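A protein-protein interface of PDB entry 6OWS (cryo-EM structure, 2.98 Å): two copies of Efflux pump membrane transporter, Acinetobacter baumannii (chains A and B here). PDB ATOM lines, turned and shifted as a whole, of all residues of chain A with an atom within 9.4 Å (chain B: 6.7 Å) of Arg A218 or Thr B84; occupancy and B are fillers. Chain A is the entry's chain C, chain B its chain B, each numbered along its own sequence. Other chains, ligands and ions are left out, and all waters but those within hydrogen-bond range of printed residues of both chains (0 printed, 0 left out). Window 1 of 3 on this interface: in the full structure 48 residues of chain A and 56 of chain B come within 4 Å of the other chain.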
ATOM      1  N   ALA A 215      17.635   9.848 -21.104  1.00  0.00           N
ATOM      2  CA  ALA A 215      18.491   9.040 -20.247  1.00  0.00           C
ATOM      3  C   ALA A 215      19.942   9.155 -20.699  1.00  0.00           C
ATOM      4  O   ALA A 215      20.216   9.062 -21.897  1.00  0.00           O
ATOM      5  CB  ALA A 215      18.046   7.587 -20.276  1.00  0.00           C
ATOM      6  N   PRO A 216      20.888   9.383 -19.782  1.00  0.00           N
ATOM      7  CA  PRO A 216      22.259   9.727 -20.187  1.00  0.00           C
ATOM      8  C   PRO A 216      23.069   8.648 -20.895  1.00  0.00           C
ATOM      9  O   PRO A 216      23.398   8.813 -22.069  1.00  0.00           O
ATOM     10  CB  PRO A 216      22.916  10.097 -18.855  1.00  0.00           C
ATOM     11  CG  PRO A 216      22.061   9.499 -17.816  1.00  0.00           C
ATOM     12  CD  PRO A 216      20.689   9.521 -18.335  1.00  0.00           C
ATOM     13  N   GLY A 217      23.356   7.528 -20.242  1.00  0.00           N
ATOM     14  CA  GLY A 217      24.223   6.525 -20.833  1.00  0.00           C
ATOM     15  C   GLY A 217      25.695   6.916 -20.864  1.00  0.00           C
ATOM     16  O   GLY A 217      26.091   8.026 -20.522  1.00  0.00           O
ATOM     17  N   ARG A 218      26.522   5.959 -21.284  1.00  0.00           N
ATOM     18  CA  ARG A 218      27.962   6.137 -21.434  1.00  0.00           C
ATOM     19  C   ARG A 218      28.383   5.730 -22.836  1.00  0.00           C
ATOM     20  O   ARG A 218      27.586   5.229 -23.624  1.00  0.00           O
ATOM     21  CB  ARG A 218      28.754   5.306 -20.424  1.00  0.00           C
ATOM     22  CG  ARG A 218      28.386   5.516 -18.991  1.00  0.00           C
ATOM     23  CD  ARG A 218      29.318   4.730 -18.101  1.00  0.00           C
ATOM     24  NE  ARG A 218      30.662   5.291 -18.090  1.00  0.00           N
ATOM     25  CZ  ARG A 218      31.068   6.209 -17.222  1.00  0.00           C
ATOM     26  NH1 ARG A 218      32.303   6.677 -17.272  1.00  0.00           N
ATOM     27  NH2 ARG A 218      30.231   6.660 -16.304  1.00  0.00           N
ATOM     28  N   LEU A 219      29.665   5.921 -23.132  1.00  0.00           N
ATOM     29  CA  LEU A 219      30.245   5.581 -24.429  1.00  0.00           C
ATOM     30  C   LEU A 219      31.381   4.599 -24.189  1.00  0.00           C
ATOM     31  O   LEU A 219      32.487   5.002 -23.834  1.00  0.00           O
ATOM     32  CB  LEU A 219      30.760   6.811 -25.146  1.00  0.00           C
ATOM     33  CG  LEU A 219      29.853   7.560 -26.099  1.00  0.00           C
ATOM     34  CD1 LEU A 219      30.661   8.639 -26.754  1.00  0.00           C
ATOM     35  CD2 LEU A 219      29.315   6.619 -27.123  1.00  0.00           C
ATOM     36  N   GLY A 220      31.127   3.322 -24.400  1.00  0.00           N
ATOM     37  CA  GLY A 220      32.172   2.355 -24.170  1.00  0.00           C
ATOM     38  C   GLY A 220      31.907   1.556 -22.921  1.00  0.00           C
ATOM     39  O   GLY A 220      32.834   1.226 -22.181  1.00  0.00           O
ATOM     40  N   ASP A 221      30.643   1.238 -22.675  1.00  0.00           N
ATOM     41  CA  ASP A 221      30.302   0.475 -21.491  1.00  0.00           C
ATOM     42  C   ASP A 221      30.703  -0.981 -21.667  1.00  0.00           C
ATOM     43  O   ASP A 221      30.959  -1.459 -22.771  1.00  0.00           O
ATOM     44  CB  ASP A 221      28.816   0.589 -21.184  1.00  0.00           C
ATOM     45  CG  ASP A 221      28.544   0.650 -19.700  1.00  0.00           C
ATOM     46  OD1 ASP A 221      29.522   0.652 -18.925  1.00  0.00           O
ATOM     47  OD2 ASP A 221      27.364   0.699 -19.303  1.00  0.00           O
ATOM     48  N   LEU A 222      30.733  -1.688 -20.556  1.00  0.00           N
ATOM     49  CA  LEU A 222      31.637  -2.815 -20.363  1.00  0.00           C
ATOM     50  C   LEU A 222      31.405  -4.087 -21.191  1.00  0.00           C
ATOM     51  O   LEU A 222      32.384  -4.802 -21.443  1.00  0.00           O
ATOM     52  CB  LEU A 222      31.693  -3.113 -18.865  1.00  0.00           C
ATOM     53  CG  LEU A 222      32.835  -3.973 -18.335  1.00  0.00           C
ATOM     54  CD1 LEU A 222      34.108  -3.582 -18.992  1.00  0.00           C
ATOM     55  CD2 LEU A 222      33.016  -3.620 -16.889  1.00  0.00           C
ATOM     56  N   ILE A 230      39.171   4.510 -24.497  1.00  0.00           N
ATOM     57  CA  ILE A 230      38.577   5.641 -23.799  1.00  0.00           C
ATOM     58  C   ILE A 230      37.100   5.373 -23.566  1.00  0.00           C
ATOM     59  O   ILE A 230      36.376   5.015 -24.500  1.00  0.00           O
ATOM     60  CB  ILE A 230      38.768   6.943 -24.590  1.00  0.00           C
ATOM     61  CG1 ILE A 230      40.244   7.167 -24.895  1.00  0.00           C
ATOM     62  CG2 ILE A 230      38.220   8.115 -23.823  1.00  0.00           C
ATOM     63  CD1 ILE A 230      40.510   8.399 -25.700  1.00  0.00           C
ATOM     64  N   THR A 231      36.656   5.544 -22.329  1.00  0.00           N
ATOM     65  CA  THR A 231      35.244   5.626 -21.997  1.00  0.00           C
ATOM     66  C   THR A 231      34.918   7.046 -21.571  1.00  0.00           C
ATOM     67  O   THR A 231      35.771   7.757 -21.043  1.00  0.00           O
ATOM     68  CB  THR A 231      34.851   4.643 -20.894  1.00  0.00           C
ATOM     69  OG1 THR A 231      33.473   4.827 -20.567  1.00  0.00           O
ATOM     70  CG2 THR A 231      35.676   4.833 -19.657  1.00  0.00           C
ATOM     71  N   ILE A 232      33.686   7.468 -21.821  1.00  0.00           N
ATOM     72  CA  ILE A 232      33.306   8.854 -21.571  1.00  0.00           C
ATOM     73  C   ILE A 232      31.792   8.935 -21.419  1.00  0.00           C
ATOM     74  O   ILE A 232      31.062   8.262 -22.153  1.00  0.00           O
ATOM     75  CB  ILE A 232      33.855   9.774 -22.678  1.00  0.00           C
ATOM     76  CG1 ILE A 232      33.575  11.237 -22.388  1.00  0.00           C
ATOM     77  CG2 ILE A 232      33.395   9.362 -24.057  1.00  0.00           C
ATOM     78  CD1 ILE A 232      34.406  12.140 -23.223  1.00  0.00           C
ATOM     79  N   PRO A 233      31.278   9.673 -20.444  1.00  0.00           N
ATOM     80  CA  PRO A 233      29.830   9.806 -20.314  1.00  0.00           C
ATOM     81  C   PRO A 233      29.251  10.698 -21.393  1.00  0.00           C
ATOM     82  O   PRO A 233      29.900  11.608 -21.905  1.00  0.00           O
ATOM     83  CB  PRO A 233      29.655  10.440 -18.934  1.00  0.00           C
ATOM     84  CG  PRO A 233      30.876  10.137 -18.235  1.00  0.00           C
ATOM     85  CD  PRO A 233      31.959  10.169 -19.246  1.00  0.00           C
ATOM     86  N   LEU A 234      27.995  10.433 -21.724  1.00  0.00           N
ATOM     87  CA  LEU A 234      27.303  11.226 -22.719  1.00  0.00           C
ATOM     88  C   LEU A 234      25.927  11.554 -22.176  1.00  0.00           C
ATOM     89  O   LEU A 234      25.349  10.777 -21.420  1.00  0.00           O
ATOM     90  CB  LEU A 234      27.219  10.480 -24.050  1.00  0.00           C
ATOM     91  CG  LEU A 234      26.790  11.222 -25.307  1.00  0.00           C
ATOM     92  CD1 LEU A 234      27.529  10.638 -26.462  1.00  0.00           C
ATOM     93  CD2 LEU A 234      25.319  11.067 -25.557  1.00  0.00           C
ATOM     94  N   SER A 235      25.417  12.718 -22.556  1.00  0.00           N
ATOM     95  CA  SER A 235      24.103  13.163 -22.116  1.00  0.00           C
ATOM     96  C   SER A 235      23.595  14.211 -23.085  1.00  0.00           C
ATOM     97  O   SER A 235      24.369  14.829 -23.815  1.00  0.00           O
ATOM     98  CB  SER A 235      24.141  13.736 -20.705  1.00  0.00           C
ATOM     99  OG  SER A 235      23.932  15.133 -20.756  1.00  0.00           O
ATOM    100  N   GLY B  51      21.036   4.278 -14.251  1.00  0.00           N
ATOM    101  CA  GLY B  51      21.442   4.947 -15.460  1.00  0.00           C
ATOM    102  C   GLY B  51      21.968   6.355 -15.269  1.00  0.00           C
ATOM    103  O   GLY B  51      22.842   6.785 -16.025  1.00  0.00           O
ATOM    104  N   ALA B  52      21.476   7.075 -14.264  1.00  0.00           N
ATOM    105  CA  ALA B  52      21.730   8.502 -14.177  1.00  0.00           C
ATOM    106  C   ALA B  52      23.063   8.801 -13.509  1.00  0.00           C
ATOM    107  O   ALA B  52      23.649   7.973 -12.808  1.00  0.00           O
ATOM    108  CB  ALA B  52      20.619   9.204 -13.411  1.00  0.00           C
ATOM    109  N   THR B  53      23.532  10.024 -13.731  1.00  0.00           N
ATOM    110  CA  THR B  53      24.791  10.492 -13.189  1.00  0.00           C
ATOM    111  C   THR B  53      24.644  10.830 -11.716  1.00  0.00           C
ATOM    112  O   THR B  53      23.542  10.997 -11.194  1.00  0.00           O
ATOM    113  CB  THR B  53      25.269  11.726 -13.937  1.00  0.00           C
ATOM    114  OG1 THR B  53      24.521  12.859 -13.490  1.00  0.00           O
ATOM    115  CG2 THR B  53      25.050  11.551 -15.415  1.00  0.00           C
ATOM    116  N   ALA B  54      25.788  10.956 -11.048  1.00  0.00           N
ATOM    117  CA  ALA B  54      25.794  11.286  -9.631  1.00  0.00           C
ATOM    118  C   ALA B  54      25.403  12.729  -9.367  1.00  0.00           C
ATOM    119  O   ALA B  54      25.105  13.069  -8.220  1.00  0.00           O
ATOM    120  CB  ALA B  54      27.171  11.013  -9.041  1.00  0.00           C
ATOM    121  N   THR B  82      28.091   9.105  -3.780  1.00  0.00           N
ATOM    122  CA  THR B  82      27.492   8.732  -5.048  1.00  0.00           C
ATOM    123  C   THR B  82      28.589   8.614  -6.086  1.00  0.00           C
ATOM    124  O   THR B  82      29.633   9.252  -5.972  1.00  0.00           O
ATOM    125  CB  THR B  82      26.459   9.747  -5.525  1.00  0.00           C
ATOM    126  OG1 THR B  82      26.139  10.660  -4.468  1.00  0.00           O
ATOM    127  CG2 THR B  82      25.216   9.039  -5.990  1.00  0.00           C
ATOM    128  N   ASP B  83      28.347   7.794  -7.097  1.00  0.00           N
ATOM    129  CA  ASP B  83      29.321   7.622  -8.160  1.00  0.00           C
ATOM    130  C   ASP B  83      28.575   7.245  -9.430  1.00  0.00           C
ATOM    131  O   ASP B  83      27.349   7.360  -9.501  1.00  0.00           O
ATOM    132  CB  ASP B  83      30.395   6.598  -7.754  1.00  0.00           C
ATOM    133  CG  ASP B  83      29.814   5.326  -7.207  1.00  0.00           C
ATOM    134  OD1 ASP B  83      28.586   5.275  -6.991  1.00  0.00           O
ATOM    135  OD2 ASP B  83      30.586   4.373  -6.991  1.00  0.00           O
ATOM    136  N   THR B  84      29.317   6.786 -10.432  1.00  0.00           N
ATOM    137  CA  THR B  84      28.794   6.574 -11.773  1.00  0.00           C
ATOM    138  C   THR B  84      27.964   5.311 -11.918  1.00  0.00           C
ATOM    139  O   THR B  84      27.391   5.096 -12.989  1.00  0.00           O
ATOM    140  CB  THR B  84      29.948   6.523 -12.769  1.00  0.00           C
ATOM    141  OG1 THR B  84      30.960   5.646 -12.266  1.00  0.00           O
ATOM    142  CG2 THR B  84      30.540   7.903 -12.963  1.00  0.00           C
ATOM    143  N   SER B  85      27.891   4.473 -10.885  1.00  0.00           N
ATOM    144  CA  SER B  85      27.200   3.195 -11.011  1.00  0.00           C
ATOM    145  C   SER B  85      25.692   3.379 -11.109  1.00  0.00           C
ATOM    146  O   SER B  85      25.006   2.582 -11.756  1.00  0.00           O
ATOM    147  CB  SER B  85      27.547   2.301  -9.829  1.00  0.00           C
ATOM    148  OG  SER B  85      27.008   2.840  -8.643  1.00  0.00           O
ATOM    149  N   GLY B  86      25.158   4.415 -10.481  1.00  0.00           N
ATOM    150  CA  GLY B  86      23.740   4.671 -10.574  1.00  0.00           C
ATOM    151  C   GLY B  86      23.026   4.477  -9.260  1.00  0.00           C
ATOM    152  O   GLY B  86      21.800   4.569  -9.189  1.00  0.00           O
ATOM    153  N   THR B  87      23.783   4.210  -8.207  1.00  0.00           N
ATOM    154  CA  THR B  87      23.222   4.039  -6.881  1.00  0.00           C
ATOM    155  C   THR B  87      23.940   4.960  -5.908  1.00  0.00           C
ATOM    156  O   THR B  87      25.074   5.385  -6.137  1.00  0.00           O
ATOM    157  CB  THR B  87      23.316   2.576  -6.418  1.00  0.00           C
ATOM    158  OG1 THR B  87      22.720   2.437  -5.122  1.00  0.00           O
ATOM    159  CG2 THR B  87      24.754   2.103  -6.365  1.00  0.00           C
ATOM    160  N   SER B 577      39.975   8.769 -15.138  1.00  0.00           N
ATOM    161  CA  SER B 577      38.571   8.419 -15.347  1.00  0.00           C
ATOM    162  C   SER B 577      38.094   8.069 -16.705  1.00  0.00           C
ATOM    163  O   SER B 577      36.924   7.906 -16.888  1.00  0.00           O
ATOM    164  CB  SER B 577      37.655   9.454 -14.802  1.00  0.00           C
ATOM    165  OG  SER B 577      38.177  10.687 -15.111  1.00  0.00           O
ATOM    166  N   ASP B 578      38.965   7.995 -17.677  1.00  0.00           N
ATOM    167  CA  ASP B 578      38.559   7.665 -18.993  1.00  0.00           C
ATOM    168  C   ASP B 578      39.174   6.402 -19.310  1.00  0.00           C
ATOM    169  O   ASP B 578      39.413   6.115 -20.392  1.00  0.00           O
ATOM    170  CB  ASP B 578      39.030   8.689 -19.971  1.00  0.00           C
ATOM    171  CG  ASP B 578      40.499   8.711 -20.123  1.00  0.00           C
ATOM    172  OD1 ASP B 578      41.169   8.186 -19.278  1.00  0.00           O
ATOM    173  OD2 ASP B 578      41.035   9.309 -21.059  1.00  0.00           O
ATOM    174  N   ALA B 615      33.016   2.764  -7.170  1.00  0.00           N
ATOM    175  CA  ALA B 615      33.034   1.652  -8.108  1.00  0.00           C
ATOM    176  C   ALA B 615      32.953   2.190  -9.523  1.00  0.00           C
ATOM    177  O   ALA B 615      32.199   3.126  -9.796  1.00  0.00           O
ATOM    178  CB  ALA B 615      31.880   0.692  -7.855  1.00  0.00           C
ATOM    179  N   GLY B 616      33.731   1.601 -10.416  1.00  0.00           N
ATOM    180  CA  GLY B 616      33.767   2.047 -11.796  1.00  0.00           C
ATOM    181  C   GLY B 616      34.658   1.131 -12.595  1.00  0.00           C
ATOM    182  O   GLY B 616      35.128   0.108 -12.102  1.00  0.00           O
ATOM    183  N   GLN B 617      34.891   1.506 -13.846  1.00  0.00           N
ATOM    184  CA  GLN B 617      35.793   0.709 -14.664  1.00  0.00           C
ATOM    185  C   GLN B 617      37.247   0.951 -14.306  1.00  0.00           C
ATOM    186  O   GLN B 617      38.075   0.051 -14.459  1.00  0.00           O
ATOM    187  CB  GLN B 617      35.580   1.006 -16.143  1.00  0.00           C
ATOM    188  CG  GLN B 617      34.425   0.273 -16.757  1.00  0.00           C
ATOM    189  CD  GLN B 617      34.370   0.449 -18.247  1.00  0.00           C
ATOM    190  OE1 GLN B 617      33.664   1.312 -18.753  1.00  0.00           O
ATOM    191  NE2 GLN B 617      35.119  -0.363 -18.961  1.00  0.00           N
ATOM    192  N   ASN B 618      37.584   2.147 -13.843  1.00  0.00           N
ATOM    193  CA  ASN B 618      38.964   2.475 -13.506  1.00  0.00           C
ATOM    194  C   ASN B 618      39.262   2.230 -12.034  1.00  0.00           C
ATOM    195  O   ASN B 618      39.890   3.051 -11.379  1.00  0.00           O
ATOM    196  CB  ASN B 618      39.217   3.927 -13.860  1.00  0.00           C
ATOM    197  CG  ASN B 618      38.172   4.836 -13.276  1.00  0.00           C
ATOM    198  OD1 ASN B 618      37.019   4.453 -13.148  1.00  0.00           O
ATOM    199  ND2 ASN B 618      38.569   6.034 -12.896  1.00  0.00           N
ATOM    200  N   LEU B 712      36.898   8.765  -6.820  1.00  0.00           N
ATOM    201  CA  LEU B 712      37.116   8.836  -8.256  1.00  0.00           C
ATOM    202  C   LEU B 712      37.493  10.254  -8.655  1.00  0.00           C
ATOM    203  O   LEU B 712      36.858  11.206  -8.198  1.00  0.00           O
ATOM    204  CB  LEU B 712      35.867   8.412  -9.000  1.00  0.00           C
ATOM    205  CG  LEU B 712      35.076   7.266  -8.390  1.00  0.00           C
ATOM    206  CD1 LEU B 712      33.791   7.115  -9.145  1.00  0.00           C
ATOM    207  CD2 LEU B 712      35.864   5.985  -8.447  1.00  0.00           C
ATOM    208  N   SER B 744      19.953   4.077 -26.905  1.00  0.00           N
ATOM    209  CA  SER B 744      21.091   3.987 -27.804  1.00  0.00           C
ATOM    210  C   SER B 744      22.335   3.521 -27.081  1.00  0.00           C
ATOM    211  O   SER B 744      23.261   3.013 -27.710  1.00  0.00           O
ATOM    212  CB  SER B 744      21.376   5.329 -28.460  1.00  0.00           C
ATOM    213  OG  SER B 744      22.755   5.467 -28.689  1.00  0.00           O
ATOM    214  N   MET B 745      22.386   3.711 -25.773  1.00  0.00           N
ATOM    215  CA  MET B 745      23.567   3.346 -25.019  1.00  0.00           C
ATOM    216  C   MET B 745      23.272   2.565 -23.756  1.00  0.00           C
ATOM    217  O   MET B 745      24.154   1.844 -23.285  1.00  0.00           O
ATOM    218  CB  MET B 745      24.373   4.595 -24.646  1.00  0.00           C
ATOM    219  CG  MET B 745      25.097   5.240 -25.803  1.00  0.00           C
ATOM    220  SD  MET B 745      25.513   6.948 -25.440  1.00  0.00           S
ATOM    221  CE  MET B 745      23.891   7.620 -25.149  1.00  0.00           C
ATOM    222  N   GLY B 746      22.075   2.674 -23.195  1.00  0.00           N
ATOM    223  CA  GLY B 746      21.709   1.913 -22.024  1.00  0.00           C
ATOM    224  C   GLY B 746      21.136   0.565 -22.400  1.00  0.00           C
ATOM    225  O   GLY B 746      20.965   0.237 -23.567  1.00  0.00           O
ATOM    226  N   ARG B 771      28.491   1.614 -30.025  1.00  0.00           N
ATOM    227  CA  ARG B 771      28.425   2.530 -28.900  1.00  0.00           C
ATOM    228  C   ARG B 771      29.806   2.725 -28.306  1.00  0.00           C
ATOM    229  O   ARG B 771      29.993   2.660 -27.089  1.00  0.00           O
ATOM    230  CB  ARG B 771      27.444   2.044 -27.843  1.00  0.00           C
ATOM    231  CG  ARG B 771      27.439   0.561 -27.669  1.00  0.00           C
ATOM    232  CD  ARG B 771      26.519   0.138 -26.556  1.00  0.00           C
ATOM    233  NE  ARG B 771      26.639  -1.288 -26.315  1.00  0.00           N
ATOM    234  CZ  ARG B 771      27.532  -1.826 -25.499  1.00  0.00           C
ATOM    235  NH1 ARG B 771      27.589  -3.135 -25.345  1.00  0.00           N
ATOM    236  NH2 ARG B 771      28.373  -1.053 -24.837  1.00  0.00           N
ATOM    237  N   ILE B 777      27.172   7.536 -32.426  1.00  0.00           N
ATOM    238  CA  ILE B 777      25.911   8.124 -32.004  1.00  0.00           C
ATOM    239  C   ILE B 777      25.443   9.150 -33.020  1.00  0.00           C
ATOM    240  O   ILE B 777      24.240   9.317 -33.236  1.00  0.00           O
ATOM    241  CB  ILE B 777      26.058   8.731 -30.601  1.00  0.00           C
ATOM    242  CG1 ILE B 777      26.646   7.699 -29.656  1.00  0.00           C
ATOM    243  CG2 ILE B 777      24.725   9.167 -30.048  1.00  0.00           C
ATOM    244  CD1 ILE B 777      25.820   6.452 -29.535  1.00  0.00           C
ATOM    245  N   GLN B 805      32.938  13.294 -10.938  1.00  0.00           N
ATOM    246  CA  GLN B 805      32.198  12.060 -11.122  1.00  0.00           C
ATOM    247  C   GLN B 805      31.701  11.475  -9.816  1.00  0.00           C
ATOM    248  O   GLN B 805      31.077  10.414  -9.827  1.00  0.00           O
ATOM    249  CB  GLN B 805      33.069  11.032 -11.839  1.00  0.00           C
ATOM    250  CG  GLN B 805      33.812  11.582 -13.019  1.00  0.00           C
ATOM    251  CD  GLN B 805      32.909  11.848 -14.185  1.00  0.00           C
ATOM    252  OE1 GLN B 805      32.561  10.940 -14.927  1.00  0.00           O
ATOM    253  NE2 GLN B 805      32.514  13.097 -14.352  1.00  0.00           N
ATOM    254  N   GLN B 806      31.958  12.135  -8.696  1.00  0.00           N
ATOM    255  CA  GLN B 806      31.579  11.603  -7.399  1.00  0.00           C
ATOM    256  C   GLN B 806      31.274  12.763  -6.473  1.00  0.00           C
ATOM    257  O   GLN B 806      32.100  13.664  -6.314  1.00  0.00           O
ATOM    258  CB  GLN B 806      32.696  10.738  -6.826  1.00  0.00           C
ATOM    259  CG  GLN B 806      32.594  10.494  -5.355  1.00  0.00           C
ATOM    260  CD  GLN B 806      33.257   9.217  -4.959  1.00  0.00           C
ATOM    261  OE1 GLN B 806      34.361   8.921  -5.395  1.00  0.00           O
ATOM    262  NE2 GLN B 806      32.580   8.434  -4.140  1.00  0.00           N
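No position is printed for both chains.
Gly B51 touches Pro A216 (O to CG, 3.3 Å). Pro A216 touches Ala B52 (CG to CA, 3.8 Å). CE of Met B745 touches O of Pro A216 (3.3 Å). Thr B84 touches Arg A218 (CB to NH2, 3.5 Å). Arg B771 touches Leu A219. CD2 of Leu A219 touches CG1 of Ile B777 (3.8 Å). NE2 of Gln B617 touches CD1 of Leu A222 (3.4 Å). Asp B578 touches Ile A230 (O to CA, 3.5 Å). Gln B617 touches Thr A231 (OE1 to OG1, 3.96 Å). Met B745 touches Leu A234.
The backbone NH (N) of Gly A220 sits at hydrogen-bond distance from the backbone carbonyl oxygen (O) of Arg B771. O of Asp B578 sits at hydrogen-bond distance from N of Thr A231, 3.4 Å away. SD of Met B745 sits close to O of Arg A218 (3.2 Å). NH2 of Arg B771 lies within hydrogen-bond range of O of Asp A221 (3.3 Å).
The backbone NH (N) of Leu A234 sits at hydrogen-bond distance from the backbone carbonyl oxygen (O) of Gly A217, 3.3 Å away. O of Leu A219 lies close to OG1 of Thr A231 (3.4 Å). N of Leu A219 lies within hydrogen-bond range of O of Ile A232 (2.9 Å).
Printed residues of chain B within 4 Å of Arg A218: Thr B84 and Met B745. Of the printed residues of chain B, Gly A220 touches Gln B617 and Arg B771. Printed residues of chain B within 4 Å of Leu A222: Gln B617. Printed residues of chain A within 4 Å of Thr B84: Arg A218 (3.5 Å). No residue of chain A comes within 4 Å of Ser B85. Of the printed residues of chain A, Gln B617 touches Gly A220 (3.5 Å), Leu A222 (3.4 Å) and Thr A231 (3.96 Å). Ser B744 touches none of the printed residues of chain A. Printed residues of chain A within 4 Å of Ile B777: Leu A219. The nearest residue of chain A that does not touch Thr B84 is Pro A233 (5.7 Å).
Of the 14 printed residues of chain A, 10 touch a printed residue of chain B. Hydrophobic or aromatic side chains of chain A within 4 Å of the printed part of chain B: Pro A216, Leu A219, Leu A222, Ile A230, Pro A233 and Leu A234. Hydrophobic or aromatic side chains of chain B within 4 Å of the printed part of chain A: Met B745 and Ile B777. Among the printed residues, 16 pairs touch across the chains.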
